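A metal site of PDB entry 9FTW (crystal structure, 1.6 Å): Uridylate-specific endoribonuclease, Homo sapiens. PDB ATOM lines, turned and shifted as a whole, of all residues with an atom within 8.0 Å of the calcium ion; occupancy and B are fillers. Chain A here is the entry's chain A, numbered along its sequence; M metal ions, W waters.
The calcium ion is bound by water W1, OE1 of Gln 250, OE2 of Glu 140, OE1 of Glu 140 and O of Ala 135.
The calcium ion has five donor atoms within binding distance.
O of Gln 250 sits at hydrogen-bond distance from N of Asp 134 (2.9 Å).
The side-chain hydroxyl of Thr 137 sits at hydrogen-bond distance from the backbone NH of Glu 140 (3.0 Å).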
ATOM      1  N   ASP A 134      15.851  -6.540  10.867  1.00  0.00           N
ATOM      2  CA  ASP A 134      14.685  -5.729  11.210  1.00  0.00           C
ATOM      3  C   ASP A 134      15.009  -4.246  11.205  1.00  0.00           C
ATOM      4  O   ASP A 134      16.107  -3.877  11.614  1.00  0.00           O
ATOM      5  CB  ASP A 134      14.082  -6.160  12.565  1.00  0.00           C
ATOM      6  CG  ASP A 134      13.381  -7.508  12.535  1.00  0.00           C
ATOM      7  OD1 ASP A 134      12.830  -7.878  11.461  1.00  0.00           O
ATOM      8  OD2 ASP A 134      13.366  -8.178  13.594  1.00  0.00           O
ATOM      9  N   ALA A 135      14.077  -3.402  10.734  1.00  0.00           N
ATOM     10  CA  ALA A 135      14.352  -1.968  10.703  1.00  0.00           C
ATOM     11  C   ALA A 135      14.324  -1.453  12.109  1.00  0.00           C
ATOM     12  O   ALA A 135      13.481  -1.836  12.929  1.00  0.00           O
ATOM     13  CB  ALA A 135      13.375  -1.191   9.875  1.00  0.00           C
ATOM     14  N   ILE A 136      15.238  -0.556  12.359  1.00  0.00           N
ATOM     15  CA  ILE A 136      15.369   0.083  13.656  1.00  0.00           C
ATOM     16  C   ILE A 136      14.699   1.416  13.483  1.00  0.00           C
ATOM     17  O   ILE A 136      15.111   2.184  12.642  1.00  0.00           O
ATOM     18  CB  ILE A 136      16.854   0.159  14.058  1.00  0.00           C
ATOM     19  CG1 ILE A 136      17.373  -1.238  14.400  1.00  0.00           C
ATOM     20  CG2 ILE A 136      17.000   1.145  15.227  1.00  0.00           C
ATOM     21  CD1 ILE A 136      18.949  -1.388  14.461  1.00  0.00           C
ATOM     22  N   THR A 137      13.677   1.705  14.288  1.00  0.00           N
ATOM     23  CA  THR A 137      12.935   2.954  14.159  1.00  0.00           C
ATOM     24  C   THR A 137      13.580   4.075  14.988  1.00  0.00           C
ATOM     25  O   THR A 137      14.390   3.807  15.905  1.00  0.00           O
ATOM     26  CB  THR A 137      11.449   2.750  14.600  1.00  0.00           C
ATOM     27  OG1 THR A 137      11.443   2.553  16.015  1.00  0.00           O
ATOM     28  CG2 THR A 137      10.752   1.598  13.876  1.00  0.00           C
ATOM     29  N   GLU A 140      12.724   3.359  18.570  1.00  0.00           N
ATOM     30  CA  GLU A 140      13.546   2.285  19.119  1.00  0.00           C
ATOM     31  C   GLU A 140      14.944   2.827  19.489  1.00  0.00           C
ATOM     32  O   GLU A 140      15.485   2.484  20.548  1.00  0.00           O
ATOM     33  CB  GLU A 140      13.654   1.096  18.118  1.00  0.00           C
ATOM     34  CG  GLU A 140      12.424   0.161  18.108  1.00  0.00           C
ATOM     35  CD  GLU A 140      12.340  -0.833  16.949  1.00  0.00           C
ATOM     36  OE1 GLU A 140      13.003  -0.610  15.913  1.00  0.00           O
ATOM     37  OE2 GLU A 140      11.626  -1.846  17.092  1.00  0.00           O
ATOM     38  N   PHE A 246      19.585  -5.488  22.154  1.00  0.00           N
ATOM     39  CA  PHE A 246      18.766  -4.698  21.232  1.00  0.00           C
ATOM     40  C   PHE A 246      19.072  -5.097  19.781  1.00  0.00           C
ATOM     41  O   PHE A 246      18.145  -5.345  19.006  1.00  0.00           O
ATOM     42  CB  PHE A 246      19.106  -3.207  21.416  1.00  0.00           C
ATOM     43  CG  PHE A 246      18.425  -2.324  20.399  1.00  0.00           C
ATOM     44  CD1 PHE A 246      17.081  -2.005  20.531  1.00  0.00           C
ATOM     45  CD2 PHE A 246      19.153  -1.728  19.388  1.00  0.00           C
ATOM     46  CE1 PHE A 246      16.454  -1.208  19.570  1.00  0.00           C
ATOM     47  CE2 PHE A 246      18.535  -0.870  18.487  1.00  0.00           C
ATOM     48  CZ  PHE A 246      17.186  -0.643  18.561  1.00  0.00           C
ATOM     49  N   HIS A 249      17.823  -8.657  18.991  1.00  0.00           N
ATOM     50  CA  HIS A 249      16.373  -8.637  18.861  1.00  0.00           C
ATOM     51  C   HIS A 249      15.956  -8.003  17.514  1.00  0.00           C
ATOM     52  O   HIS A 249      14.945  -8.400  16.935  1.00  0.00           O
ATOM     53  CB  HIS A 249      15.716  -7.871  20.033  1.00  0.00           C
ATOM     54  CG  HIS A 249      14.233  -7.745  19.918  1.00  0.00           C
ATOM     55  ND1 HIS A 249      13.389  -8.837  20.108  1.00  0.00           N
ATOM     56  CD2 HIS A 249      13.481  -6.673  19.563  1.00  0.00           C
ATOM     57  CE1 HIS A 249      12.163  -8.396  19.899  1.00  0.00           C
ATOM     58  NE2 HIS A 249      12.175  -7.107  19.559  1.00  0.00           N
ATOM     59  N   GLN A 250      16.730  -7.001  17.029  1.00  0.00           N
ATOM     60  CA  GLN A 250      16.474  -6.350  15.737  1.00  0.00           C
ATOM     61  C   GLN A 250      17.127  -7.124  14.550  1.00  0.00           C
ATOM     62  O   GLN A 250      17.185  -6.588  13.435  1.00  0.00           O
ATOM     63  CB  GLN A 250      16.958  -4.889  15.772  1.00  0.00           C
ATOM     64  CG  GLN A 250      16.340  -4.050  16.906  1.00  0.00           C
ATOM     65  CD  GLN A 250      14.874  -3.758  16.745  1.00  0.00           C
ATOM     66  OE1 GLN A 250      14.362  -3.583  15.624  1.00  0.00           O
ATOM     67  NE2 GLN A 250      14.155  -3.676  17.859  1.00  0.00           N
ATOM     68  N   ASN A 251      17.580  -8.383  14.793  1.00  0.00           N
ATOM     69  CA  ASN A 251      18.197  -9.273  13.809  1.00  0.00           C
ATOM     70  C   ASN A 251      19.332  -8.628  13.013  1.00  0.00           C
ATOM     71  O   ASN A 251      19.530  -8.954  11.864  1.00  0.00           O
ATOM     72  CB  ASN A 251      17.127  -9.879  12.873  1.00  0.00           C
ATOM     73  CG  ASN A 251      16.103 -10.697  13.625  1.00  0.00           C
ATOM     74  OD1 ASN A 251      14.913 -10.362  13.651  1.00  0.00           O
ATOM     75  ND2 ASN A 251      16.529 -11.805  14.239  1.00  0.00           N
ATOM     76  N   ARG A 252      20.137  -7.757  13.654  1.00  0.00           N
ATOM     77  CA  ARG A 252      21.297  -7.176  13.002  1.00  0.00           C
ATOM     78  C   ARG A 252      22.534  -8.049  13.204  1.00  0.00           C
ATOM     79  O   ARG A 252      23.440  -8.000  12.377  1.00  0.00           O
ATOM     80  CB  ARG A 252      21.561  -5.730  13.479  1.00  0.00           C
ATOM     81  CG  ARG A 252      20.416  -4.748  13.204  1.00  0.00           C
ATOM     82  CD  ARG A 252      19.948  -4.643  11.747  1.00  0.00           C
ATOM     83  NE  ARG A 252      19.316  -3.352  11.450  1.00  0.00           N
ATOM     84  CZ  ARG A 252      19.967  -2.224  11.133  1.00  0.00           C
ATOM     85  NH1 ARG A 252      21.286  -2.214  11.021  1.00  0.00           N
ATOM     86  NH2 ARG A 252      19.287  -1.101  10.902  1.00  0.00           N
HETATM   87 CA    CA M   1      12.298  -2.758  14.959  1.00  0.00          CA
HETATM   88  O   HOH W   1      11.501  -4.560  16.183  1.00  0.00           O
